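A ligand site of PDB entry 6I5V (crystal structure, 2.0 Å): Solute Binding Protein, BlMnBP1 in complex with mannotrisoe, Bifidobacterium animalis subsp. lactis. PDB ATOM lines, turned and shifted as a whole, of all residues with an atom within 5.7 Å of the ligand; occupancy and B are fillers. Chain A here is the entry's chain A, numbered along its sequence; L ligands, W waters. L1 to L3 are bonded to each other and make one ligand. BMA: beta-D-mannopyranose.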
ATOM      1  N   ASN A  28      -9.789  33.126  15.651  1.00  0.00           N
ATOM      2  CA  ASN A  28     -11.058  33.496  16.272  1.00  0.00           C
ATOM      3  C   ASN A  28     -10.907  33.974  17.707  1.00  0.00           C
ATOM      4  O   ASN A  28     -11.881  34.480  18.280  1.00  0.00           O
ATOM      5  CB  ASN A  28     -12.035  32.297  16.251  1.00  0.00           C
ATOM      6  CG  ASN A  28     -11.497  31.074  17.020  1.00  0.00           C
ATOM      7  OD1 ASN A  28     -10.319  30.788  16.952  1.00  0.00           O
ATOM      8  ND2 ASN A  28     -12.365  30.371  17.770  1.00  0.00           N
ATOM      9  N   ARG A  29      -9.744  33.799  18.335  1.00  0.00           N
ATOM     10  CA  ARG A  29      -9.603  34.079  19.756  1.00  0.00           C
ATOM     11  C   ARG A  29      -9.314  35.569  19.995  1.00  0.00           C
ATOM     12  O   ARG A  29      -8.227  35.965  20.398  1.00  0.00           O
ATOM     13  CB  ARG A  29      -8.531  33.183  20.365  1.00  0.00           C
ATOM     14  CG  ARG A  29      -8.802  31.678  20.154  1.00  0.00           C
ATOM     15  CD  ARG A  29     -10.071  31.209  20.877  1.00  0.00           C
ATOM     16  NE  ARG A  29     -10.102  31.690  22.270  1.00  0.00           N
ATOM     17  CZ  ARG A  29      -9.696  30.977  23.319  1.00  0.00           C
ATOM     18  NH1 ARG A  29      -9.742  31.501  24.529  1.00  0.00           N
ATOM     19  NH2 ARG A  29      -9.262  29.743  23.170  1.00  0.00           N
ATOM     20  N   THR A  30     -10.352  36.378  19.802  1.00  0.00           N
ATOM     21  CA  THR A  30     -10.299  37.797  20.154  1.00  0.00           C
ATOM     22  C   THR A  30      -9.939  38.004  21.622  1.00  0.00           C
ATOM     23  O   THR A  30      -9.268  38.988  21.984  1.00  0.00           O
ATOM     24  CB  THR A  30     -11.657  38.454  19.864  1.00  0.00           C
ATOM     25  OG1 THR A  30     -12.693  37.717  20.522  1.00  0.00           O
ATOM     26  CG2 THR A  30     -11.948  38.527  18.327  1.00  0.00           C
ATOM     27  N   ASP A  31     -10.416  37.123  22.510  1.00  0.00           N
ATOM     28  CA  ASP A  31     -10.124  37.283  23.927  1.00  0.00           C
ATOM     29  C   ASP A  31      -8.630  37.193  24.194  1.00  0.00           C
ATOM     30  O   ASP A  31      -8.078  37.993  24.961  1.00  0.00           O
ATOM     31  CB  ASP A  31     -10.909  36.264  24.770  1.00  0.00           C
ATOM     32  CG  ASP A  31     -10.664  34.786  24.371  1.00  0.00           C
ATOM     33  OD1 ASP A  31     -10.200  34.477  23.241  1.00  0.00           O
ATOM     34  OD2 ASP A  31     -11.003  33.900  25.205  1.00  0.00           O
ATOM     35  N   ASP A  63     -10.833  38.479  14.753  1.00  0.00           N
ATOM     36  CA  ASP A  63     -12.101  39.027  14.320  1.00  0.00           C
ATOM     37  C   ASP A  63     -13.203  38.312  15.088  1.00  0.00           C
ATOM     38  O   ASP A  63     -13.233  37.082  15.169  1.00  0.00           O
ATOM     39  CB  ASP A  63     -12.247  38.834  12.812  1.00  0.00           C
ATOM     40  CG  ASP A  63     -13.306  39.758  12.199  1.00  0.00           C
ATOM     41  OD1 ASP A  63     -14.450  39.814  12.723  1.00  0.00           O
ATOM     42  OD2 ASP A  63     -12.976  40.408  11.192  1.00  0.00           O
ATOM     43  N   SER A  64     -14.094  39.112  15.680  1.00  0.00           N
ATOM     44  CA  SER A  64     -15.200  38.558  16.430  1.00  0.00           C
ATOM     45  C   SER A  64     -16.128  37.746  15.542  1.00  0.00           C
ATOM     46  O   SER A  64     -16.637  36.706  15.956  1.00  0.00           O
ATOM     47  CB  SER A  64     -15.948  39.696  17.125  1.00  0.00           C
ATOM     48  OG  SER A  64     -16.761  39.147  18.152  1.00  0.00           O
ATOM     49  N   ASN A  65     -16.305  38.160  14.299  1.00  0.00           N
ATOM     50  CA  ASN A  65     -17.211  37.489  13.379  1.00  0.00           C
ATOM     51  C   ASN A  65     -16.444  36.495  12.510  1.00  0.00           C
ATOM     52  O   ASN A  65     -16.506  36.534  11.272  1.00  0.00           O
ATOM     53  CB  ASN A  65     -17.923  38.554  12.544  1.00  0.00           C
ATOM     54  CG  ASN A  65     -19.347  38.178  12.203  1.00  0.00           C
ATOM     55  OD1 ASN A  65     -19.655  37.883  11.046  1.00  0.00           O
ATOM     56  ND2 ASN A  65     -20.247  38.232  13.214  1.00  0.00           N
ATOM     57  N   TYR A  66     -15.720  35.593  13.157  1.00  0.00           N
ATOM     58  CA  TYR A  66     -14.578  34.966  12.489  1.00  0.00           C
ATOM     59  C   TYR A  66     -14.998  34.161  11.255  1.00  0.00           C
ATOM     60  O   TYR A  66     -14.401  34.297  10.177  1.00  0.00           O
ATOM     61  CB  TYR A  66     -13.767  34.089  13.464  1.00  0.00           C
ATOM     62  CG  TYR A  66     -12.618  33.455  12.753  1.00  0.00           C
ATOM     63  CD1 TYR A  66     -11.409  34.117  12.593  1.00  0.00           C
ATOM     64  CD2 TYR A  66     -12.777  32.239  12.150  1.00  0.00           C
ATOM     65  CE1 TYR A  66     -10.391  33.560  11.870  1.00  0.00           C
ATOM     66  CE2 TYR A  66     -11.769  31.665  11.440  1.00  0.00           C
ATOM     67  CZ  TYR A  66     -10.567  32.324  11.301  1.00  0.00           C
ATOM     68  OH  TYR A  66      -9.560  31.762  10.549  1.00  0.00           O
ATOM     69  N   LYS A 117      -9.370  17.108   8.325  1.00  0.00           N
ATOM     70  CA  LYS A 117      -9.286  18.187   7.308  1.00  0.00           C
ATOM     71  C   LYS A 117      -8.300  17.759   6.222  1.00  0.00           C
ATOM     72  O   LYS A 117      -7.164  18.225   6.150  1.00  0.00           O
ATOM     73  CB  LYS A 117      -8.885  19.600   7.976  1.00  0.00           C
ATOM     74  CG  LYS A 117      -9.913  20.098   9.050  1.00  0.00           C
ATOM     75  CD  LYS A 117     -11.148  20.796   8.444  1.00  0.00           C
ATOM     76  CE  LYS A 117     -12.334  20.961   9.399  1.00  0.00           C
ATOM     77  NZ  LYS A 117     -12.063  21.869  10.536  1.00  0.00           N
ATOM     78  N   ASN A 128      -6.145  22.655  16.283  1.00  0.00           N
ATOM     79  CA  ASN A 128      -5.404  23.318  17.347  1.00  0.00           C
ATOM     80  C   ASN A 128      -5.669  22.736  18.725  1.00  0.00           C
ATOM     81  O   ASN A 128      -5.093  23.202  19.714  1.00  0.00           O
ATOM     82  CB  ASN A 128      -5.703  24.819  17.352  1.00  0.00           C
ATOM     83  CG  ASN A 128      -7.098  25.151  17.862  1.00  0.00           C
ATOM     84  OD1 ASN A 128      -7.915  24.278  18.193  1.00  0.00           O
ATOM     85  ND2 ASN A 128      -7.384  26.471  17.935  1.00  0.00           N
ATOM     86  N   VAL A 131     -11.476  18.481  21.093  1.00  0.00           N
ATOM     87  CA  VAL A 131     -12.549  18.869  21.999  1.00  0.00           C
ATOM     88  C   VAL A 131     -13.651  17.811  22.021  1.00  0.00           C
ATOM     89  O   VAL A 131     -14.024  17.236  20.982  1.00  0.00           O
ATOM     90  CB  VAL A 131     -13.115  20.250  21.622  1.00  0.00           C
ATOM     91  CG1 VAL A 131     -12.031  21.336  21.815  1.00  0.00           C
ATOM     92  CG2 VAL A 131     -13.621  20.264  20.165  1.00  0.00           C
ATOM     93  N   GLU A 179     -25.062  34.740  18.958  1.00  0.00           N
ATOM     94  CA  GLU A 179     -23.848  34.162  18.362  1.00  0.00           C
ATOM     95  C   GLU A 179     -24.228  33.029  17.401  1.00  0.00           C
ATOM     96  O   GLU A 179     -24.538  31.908  17.838  1.00  0.00           O
ATOM     97  CB  GLU A 179     -22.906  33.629  19.447  1.00  0.00           C
ATOM     98  CG  GLU A 179     -22.289  34.677  20.392  1.00  0.00           C
ATOM     99  CD  GLU A 179     -21.565  35.851  19.669  1.00  0.00           C
ATOM    100  OE1 GLU A 179     -20.732  35.612  18.776  1.00  0.00           O
ATOM    101  OE2 GLU A 179     -21.820  37.011  20.025  1.00  0.00           O
ATOM    102  N   TRP A 181     -22.417  31.065  15.805  1.00  0.00           N
ATOM    103  CA  TRP A 181     -21.642  29.832  16.001  1.00  0.00           C
ATOM    104  C   TRP A 181     -22.141  29.039  17.206  1.00  0.00           C
ATOM    105  O   TRP A 181     -21.979  27.804  17.244  1.00  0.00           O
ATOM    106  CB  TRP A 181     -20.153  30.178  16.132  1.00  0.00           C
ATOM    107  CG  TRP A 181     -19.886  31.172  17.261  1.00  0.00           C
ATOM    108  CD1 TRP A 181     -19.791  32.527  17.158  1.00  0.00           C
ATOM    109  CD2 TRP A 181     -19.742  30.858  18.658  1.00  0.00           C
ATOM    110  NE1 TRP A 181     -19.612  33.089  18.415  1.00  0.00           N
ATOM    111  CE2 TRP A 181     -19.567  32.088  19.348  1.00  0.00           C
ATOM    112  CE3 TRP A 181     -19.742  29.661  19.397  1.00  0.00           C
ATOM    113  CZ2 TRP A 181     -19.405  32.162  20.722  1.00  0.00           C
ATOM    114  CZ3 TRP A 181     -19.616  29.740  20.797  1.00  0.00           C
ATOM    115  CH2 TRP A 181     -19.427  30.968  21.438  1.00  0.00           C
ATOM    116  N   GLN A 188     -23.001  19.637  16.564  1.00  0.00           N
ATOM    117  CA  GLN A 188     -21.899  18.823  17.060  1.00  0.00           C
ATOM    118  C   GLN A 188     -22.358  17.656  17.952  1.00  0.00           C
ATOM    119  O   GLN A 188     -21.508  16.931  18.450  1.00  0.00           O
ATOM    120  CB  GLN A 188     -20.919  19.748  17.810  1.00  0.00           C
ATOM    121  CG  GLN A 188     -20.500  20.979  17.047  1.00  0.00           C
ATOM    122  CD  GLN A 188     -19.625  21.934  17.870  1.00  0.00           C
ATOM    123  OE1 GLN A 188     -19.448  21.771  19.080  1.00  0.00           O
ATOM    124  NE2 GLN A 188     -19.037  22.887  17.186  1.00  0.00           N
ATOM    125  N   TRP A 248     -22.562  36.984  24.644  1.00  0.00           N
ATOM    126  CA  TRP A 248     -21.634  35.889  24.888  1.00  0.00           C
ATOM    127  C   TRP A 248     -20.560  36.258  25.921  1.00  0.00           C
ATOM    128  O   TRP A 248     -20.216  35.429  26.766  1.00  0.00           O
ATOM    129  CB  TRP A 248     -21.015  35.456  23.569  1.00  0.00           C
ATOM    130  CG  TRP A 248     -19.744  34.682  23.675  1.00  0.00           C
ATOM    131  CD1 TRP A 248     -18.502  35.054  23.236  1.00  0.00           C
ATOM    132  CD2 TRP A 248     -19.603  33.388  24.240  1.00  0.00           C
ATOM    133  NE1 TRP A 248     -17.587  34.050  23.478  1.00  0.00           N
ATOM    134  CE2 TRP A 248     -18.244  33.017  24.109  1.00  0.00           C
ATOM    135  CE3 TRP A 248     -20.494  32.495  24.856  1.00  0.00           C
ATOM    136  CZ2 TRP A 248     -17.754  31.795  24.576  1.00  0.00           C
ATOM    137  CZ3 TRP A 248     -20.010  31.272  25.316  1.00  0.00           C
ATOM    138  CH2 TRP A 248     -18.642  30.938  25.166  1.00  0.00           C
ATOM    139  N   GLU A 249     -19.988  37.453  25.857  1.00  0.00           N
ATOM    140  CA  GLU A 249     -18.902  37.744  26.786  1.00  0.00           C
ATOM    141  C   GLU A 249     -19.422  37.781  28.221  1.00  0.00           C
ATOM    142  O   GLU A 249     -18.851  37.131  29.123  1.00  0.00           O
ATOM    143  CB  GLU A 249     -18.215  39.053  26.403  1.00  0.00           C
ATOM    144  CG  GLU A 249     -16.727  39.005  26.636  1.00  0.00           C
ATOM    145  CD  GLU A 249     -16.050  37.895  25.845  1.00  0.00           C
ATOM    146  OE1 GLU A 249     -15.390  37.075  26.493  1.00  0.00           O
ATOM    147  OE2 GLU A 249     -16.160  37.850  24.591  1.00  0.00           O
ATOM    148  N   LYS A 252     -20.051  34.334  30.273  1.00  0.00           N
ATOM    149  CA  LYS A 252     -18.974  33.642  30.974  1.00  0.00           C
ATOM    150  C   LYS A 252     -19.005  33.990  32.458  1.00  0.00           C
ATOM    151  O   LYS A 252     -19.157  33.116  33.299  1.00  0.00           O
ATOM    152  CB  LYS A 252     -17.621  34.012  30.358  1.00  0.00           C
ATOM    153  CG  LYS A 252     -17.531  33.734  28.847  1.00  0.00           C
ATOM    154  CD  LYS A 252     -16.302  34.390  28.205  1.00  0.00           C
ATOM    155  CE  LYS A 252     -16.312  34.221  26.701  1.00  0.00           C
ATOM    156  NZ  LYS A 252     -14.927  34.505  26.124  1.00  0.00           N
ATOM    157  N   TRP A 268     -13.778  23.046  24.904  1.00  0.00           N
ATOM    158  CA  TRP A 268     -12.966  24.253  24.922  1.00  0.00           C
ATOM    159  C   TRP A 268     -13.557  25.306  25.857  1.00  0.00           C
ATOM    160  O   TRP A 268     -12.827  26.111  26.446  1.00  0.00           O
ATOM    161  CB  TRP A 268     -12.855  24.825  23.511  1.00  0.00           C
ATOM    162  CG  TRP A 268     -14.180  25.051  22.917  1.00  0.00           C
ATOM    163  CD1 TRP A 268     -14.913  24.152  22.215  1.00  0.00           C
ATOM    164  CD2 TRP A 268     -14.960  26.230  22.987  1.00  0.00           C
ATOM    165  NE1 TRP A 268     -16.108  24.696  21.844  1.00  0.00           N
ATOM    166  CE2 TRP A 268     -16.163  25.980  22.294  1.00  0.00           C
ATOM    167  CE3 TRP A 268     -14.755  27.511  23.548  1.00  0.00           C
ATOM    168  CZ2 TRP A 268     -17.157  26.925  22.170  1.00  0.00           C
ATOM    169  CZ3 TRP A 268     -15.727  28.443  23.410  1.00  0.00           C
ATOM    170  CH2 TRP A 268     -16.915  28.155  22.730  1.00  0.00           C
ATOM    171  N   GLN A 272     -12.626  28.852  29.837  1.00  0.00           N
ATOM    172  CA  GLN A 272     -13.069  30.214  29.631  1.00  0.00           C
ATOM    173  C   GLN A 272     -14.122  30.595  30.666  1.00  0.00           C
ATOM    174  O   GLN A 272     -14.160  31.744  31.129  1.00  0.00           O
ATOM    175  CB  GLN A 272     -13.622  30.423  28.219  1.00  0.00           C
ATOM    176  CG  GLN A 272     -12.645  30.177  27.073  1.00  0.00           C
ATOM    177  CD  GLN A 272     -13.228  30.556  25.727  1.00  0.00           C
ATOM    178  OE1 GLN A 272     -14.173  31.357  25.632  1.00  0.00           O
ATOM    179  NE2 GLN A 272     -12.656  30.008  24.660  1.00  0.00           N
ATOM    180  N   ALA A 301     -13.506  15.678  18.417  1.00  0.00           N
ATOM    181  CA  ALA A 301     -13.262  16.291  17.125  1.00  0.00           C
ATOM    182  C   ALA A 301     -12.325  17.467  17.327  1.00  0.00           C
ATOM    183  O   ALA A 301     -11.995  17.847  18.456  1.00  0.00           O
ATOM    184  CB  ALA A 301     -14.561  16.716  16.440  1.00  0.00           C
ATOM    185  N   GLY A 302     -11.877  18.030  16.203  1.00  0.00           N
ATOM    186  CA  GLY A 302     -11.009  19.171  16.248  1.00  0.00           C
ATOM    187  C   GLY A 302     -11.787  20.463  16.532  1.00  0.00           C
ATOM    188  O   GLY A 302     -12.871  20.701  16.007  1.00  0.00           O
ATOM    189  N   ASP A 303     -11.216  21.267  17.401  1.00  0.00           N
ATOM    190  CA  ASP A 303     -11.499  22.701  17.360  1.00  0.00           C
ATOM    191  C   ASP A 303     -10.862  23.272  16.087  1.00  0.00           C
ATOM    192  O   ASP A 303     -10.251  22.547  15.288  1.00  0.00           O
ATOM    193  CB  ASP A 303     -10.943  23.356  18.623  1.00  0.00           C
ATOM    194  CG  ASP A 303     -11.591  24.701  18.919  1.00  0.00           C
ATOM    195  OD1 ASP A 303     -12.080  25.364  17.989  1.00  0.00           O
ATOM    196  OD2 ASP A 303     -11.606  25.065  20.100  1.00  0.00           O
ATOM    197  N   TYR A 304     -10.973  24.588  15.895  1.00  0.00           N
ATOM    198  CA  TYR A 304     -10.463  25.191  14.671  1.00  0.00           C
ATOM    199  C   TYR A 304      -9.112  24.609  14.256  1.00  0.00           C
ATOM    200  O   TYR A 304      -8.237  24.371  15.099  1.00  0.00           O
ATOM    201  CB  TYR A 304     -10.365  26.688  14.876  1.00  0.00           C
ATOM    202  CG  TYR A 304     -11.594  27.395  14.392  1.00  0.00           C
ATOM    203  CD1 TYR A 304     -11.871  27.446  13.032  1.00  0.00           C
ATOM    204  CD2 TYR A 304     -12.461  28.032  15.273  1.00  0.00           C
ATOM    205  CE1 TYR A 304     -12.973  28.065  12.566  1.00  0.00           C
ATOM    206  CE2 TYR A 304     -13.571  28.713  14.796  1.00  0.00           C
ATOM    207  CZ  TYR A 304     -13.792  28.723  13.417  1.00  0.00           C
ATOM    208  OH  TYR A 304     -14.867  29.324  12.845  1.00  0.00           O
ATOM    209  N   ASN A 388     -21.662  22.873   9.818  1.00  0.00           N
ATOM    210  CA  ASN A 388     -20.849  23.916   9.207  1.00  0.00           C
ATOM    211  C   ASN A 388     -20.749  25.153  10.083  1.00  0.00           C
ATOM    212  O   ASN A 388     -19.647  25.646  10.395  1.00  0.00           O
ATOM    213  CB  ASN A 388     -21.450  24.406   7.881  1.00  0.00           C
ATOM    214  CG  ASN A 388     -21.378  23.401   6.790  1.00  0.00           C
ATOM    215  OD1 ASN A 388     -20.834  22.320   6.979  1.00  0.00           O
ATOM    216  ND2 ASN A 388     -21.933  23.741   5.628  1.00  0.00           N
ATOM    217  N   GLY A 389     -21.901  25.689  10.461  1.00  0.00           N
ATOM    218  CA  GLY A 389     -22.041  27.032  10.986  1.00  0.00           C
ATOM    219  C   GLY A 389     -23.219  27.735  10.321  1.00  0.00           C
ATOM    220  O   GLY A 389     -23.357  28.962  10.463  1.00  0.00           O
HETATM  221  C1  BMA L   1     -13.873  34.938  22.315  1.00  0.00           C
HETATM  222  C2  BMA L   1     -13.705  33.505  22.809  1.00  0.00           C
HETATM  223  C3  BMA L   1     -13.742  32.545  21.621  1.00  0.00           C
HETATM  224  C4  BMA L   1     -15.008  32.739  20.795  1.00  0.00           C
HETATM  225  C5  BMA L   1     -15.113  34.206  20.372  1.00  0.00           C
HETATM  226  C6  BMA L   1     -16.386  34.460  19.600  1.00  0.00           C
HETATM  227  O1  BMA L   1     -13.959  35.794  23.473  1.00  0.00           O
HETATM  228  O2  BMA L   1     -14.815  33.155  23.593  1.00  0.00           O
HETATM  229  O3  BMA L   1     -13.677  31.201  22.077  1.00  0.00           O
HETATM  230  O4  BMA L   1     -14.997  31.993  19.625  1.00  0.00           O
HETATM  231  O5  BMA L   1     -15.063  35.064  21.554  1.00  0.00           O
HETATM  232  O6  BMA L   1     -16.423  35.783  19.179  1.00  0.00           O
HETATM  233  C1  BMA L   2     -15.454  30.641  19.645  1.00  0.00           C
HETATM  234  C2  BMA L   2     -16.166  30.392  18.270  1.00  0.00           C
HETATM  235  C3  BMA L   2     -16.477  28.901  18.100  1.00  0.00           C
HETATM  236  C4  BMA L   2     -15.206  28.013  18.369  1.00  0.00           C
HETATM  237  C5  BMA L   2     -14.600  28.370  19.743  1.00  0.00           C
HETATM  238  C6  BMA L   2     -13.290  27.575  20.007  1.00  0.00           C
HETATM  239  O2  BMA L   2     -15.335  30.767  17.161  1.00  0.00           O
HETATM  240  O3  BMA L   2     -17.066  28.614  16.795  1.00  0.00           O
HETATM  241  O4  BMA L   2     -15.540  26.646  18.454  1.00  0.00           O
HETATM  242  O5  BMA L   2     -14.344  29.807  19.842  1.00  0.00           O
HETATM  243  O6  BMA L   2     -12.303  27.880  19.019  1.00  0.00           O
HETATM  244  C1  BMA L   3     -15.275  25.929  17.311  1.00  0.00           C
HETATM  245  C2  BMA L   3     -15.317  24.453  17.772  1.00  0.00           C
HETATM  246  C3  BMA L   3     -14.956  23.594  16.570  1.00  0.00           C
HETATM  247  C4  BMA L   3     -15.854  23.955  15.370  1.00  0.00           C
HETATM  248  C5  BMA L   3     -15.835  25.490  15.117  1.00  0.00           C
HETATM  249  C6  BMA L   3     -16.728  25.938  13.966  1.00  0.00           C
HETATM  250  O2  BMA L   3     -16.606  24.074  18.172  1.00  0.00           O
HETATM  251  O3  BMA L   3     -15.012  22.141  16.841  1.00  0.00           O
HETATM  252  O4  BMA L   3     -15.416  23.281  14.157  1.00  0.00           O
HETATM  253  O5  BMA L   3     -16.253  26.119  16.314  1.00  0.00           O
HETATM  254  O6  BMA L   3     -18.034  25.493  14.190  1.00  0.00           O
HETATM  255  O   HOH W   1      -9.672  28.185  20.353  1.00  0.00           O
HETATM  256  O   HOH W   2     -16.038  33.386  16.336  1.00  0.00           O
HETATM  257  O   HOH W   3     -16.692  22.146  20.179  1.00  0.00           O
HETATM  258  O   HOH W   4     -13.358  23.571  12.131  1.00  0.00           O
HETATM  259  O   HOH W   5     -17.432  21.782  13.394  1.00  0.00           O
HETATM  260  O   HOH W   6     -16.782  20.185  17.514  1.00  0.00           O
HETATM  261  O   HOH W   7     -20.041  25.915  16.295  1.00  0.00           O
HETATM  262  O   HOH W   8     -17.035  30.239  14.438  1.00  0.00           O
HETATM  263  O   HOH W   9     -14.255  35.151  17.256  1.00  0.00           O
HETATM  264  O   HOH W  10     -18.612  26.135  19.007  1.00  0.00           O
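The side-chain amide oxygen of Gln 272 sits at hydrogen-bond distance from the side-chain amino group of Lys 252 (3.3 Å).
The side-chain carboxylate (OE1) of Glu 179 lies within hydrogen-bond range of the indole nitrogen (NE1) of Trp 181, at 2.8 Å.
NZ of Lys 252 is in salt-bridge range of OE1 of Glu 249 (2.6 Å).
The side-chain carboxylate (OD2) of Asp 31 lies within salt-bridge range of the guanidinium group (NH1) of Arg 29, 2.8 Å away.
The side-chain amide nitrogen of Gln 272 sits close to the guanidinium group of Arg 29, at 3.3 Å.
O of Tyr 304 sits at hydrogen-bond distance from N of Asn 128 (3.0 Å).
Water W6 lies within hydrogen-bond range of an oxygen (O3) of BMA L3 (2.7 Å) and the side-chain amide oxygen of Gln 188 (3.5 Å).
Water W3 lies within hydrogen-bond range of O2 of BMA L3 (2.8 Å), OE1 of Gln 188 (3.0 Å) and NE1 of Trp 268 (3.1 Å).
Water W2 lies within hydrogen-bond range of an oxygen (O2) of BMA L2 and the backbone carbonyl oxygen of Ser 64.
Water W8 bridges OH of Tyr 304 and O3 of BMA L2.
Water W4 lies within hydrogen-bond range of NZ of Lys 117 (2.7 Å) and O4 of BMA L3 (2.9 Å).
Water W7 lies within hydrogen-bond range of O of Trp 181, O6 of BMA L3 and NE2 of Gln 188.
An oxygen (O2) of BMA L3 lies within hydrogen-bond range of the side-chain amide nitrogen of Gln 188 (2.9 Å).
OE1 of Gln 272 lies within hydrogen-bond range of O2 of BMA L1, 2.8 Å away.
ND2 of Asn 28 sits at hydrogen-bond distance from O6 of BMA L2 (2.8 Å).
The side-chain carboxylate of Glu 249 is in hydrogen-bond range of an oxygen (O1) of BMA L1 (3.2 Å).
An oxygen (O6) of BMA L2 lies within hydrogen-bond range of the side-chain carboxylate (OD1) of Asp 303 (2.7 Å).
O2 of BMA L1 is in hydrogen-bond range of NZ of Lys 252 (2.9 Å).
An oxygen (O6) of BMA L1 is in hydrogen-bond range of the backbone carbonyl oxygen of Ser 64 (3.4 Å).
The backbone carbonyl oxygen (O) of Gly 302 is in hydrogen-bond range of an oxygen (O3) of BMA L3, at 2.7 Å.
The indole nitrogen (NE1) of Trp 248 sits at hydrogen-bond distance from an oxygen (O2) of BMA L1 (2.9 Å).
Residues that only touch the ligand: Arg 29, Thr 30, Asp 31, Trp 181, Trp 268 and Tyr 304.
Hydrophobic or aromatic side chains within 4 Å of the ligand: Trp 181, Trp 248, Trp 268 and Tyr 304.
Of the 25 residues printed, 15 come within 4 Å of the ligand.
The nearest printed residue that does not touch the ligand is Val 131 (4.1 Å).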
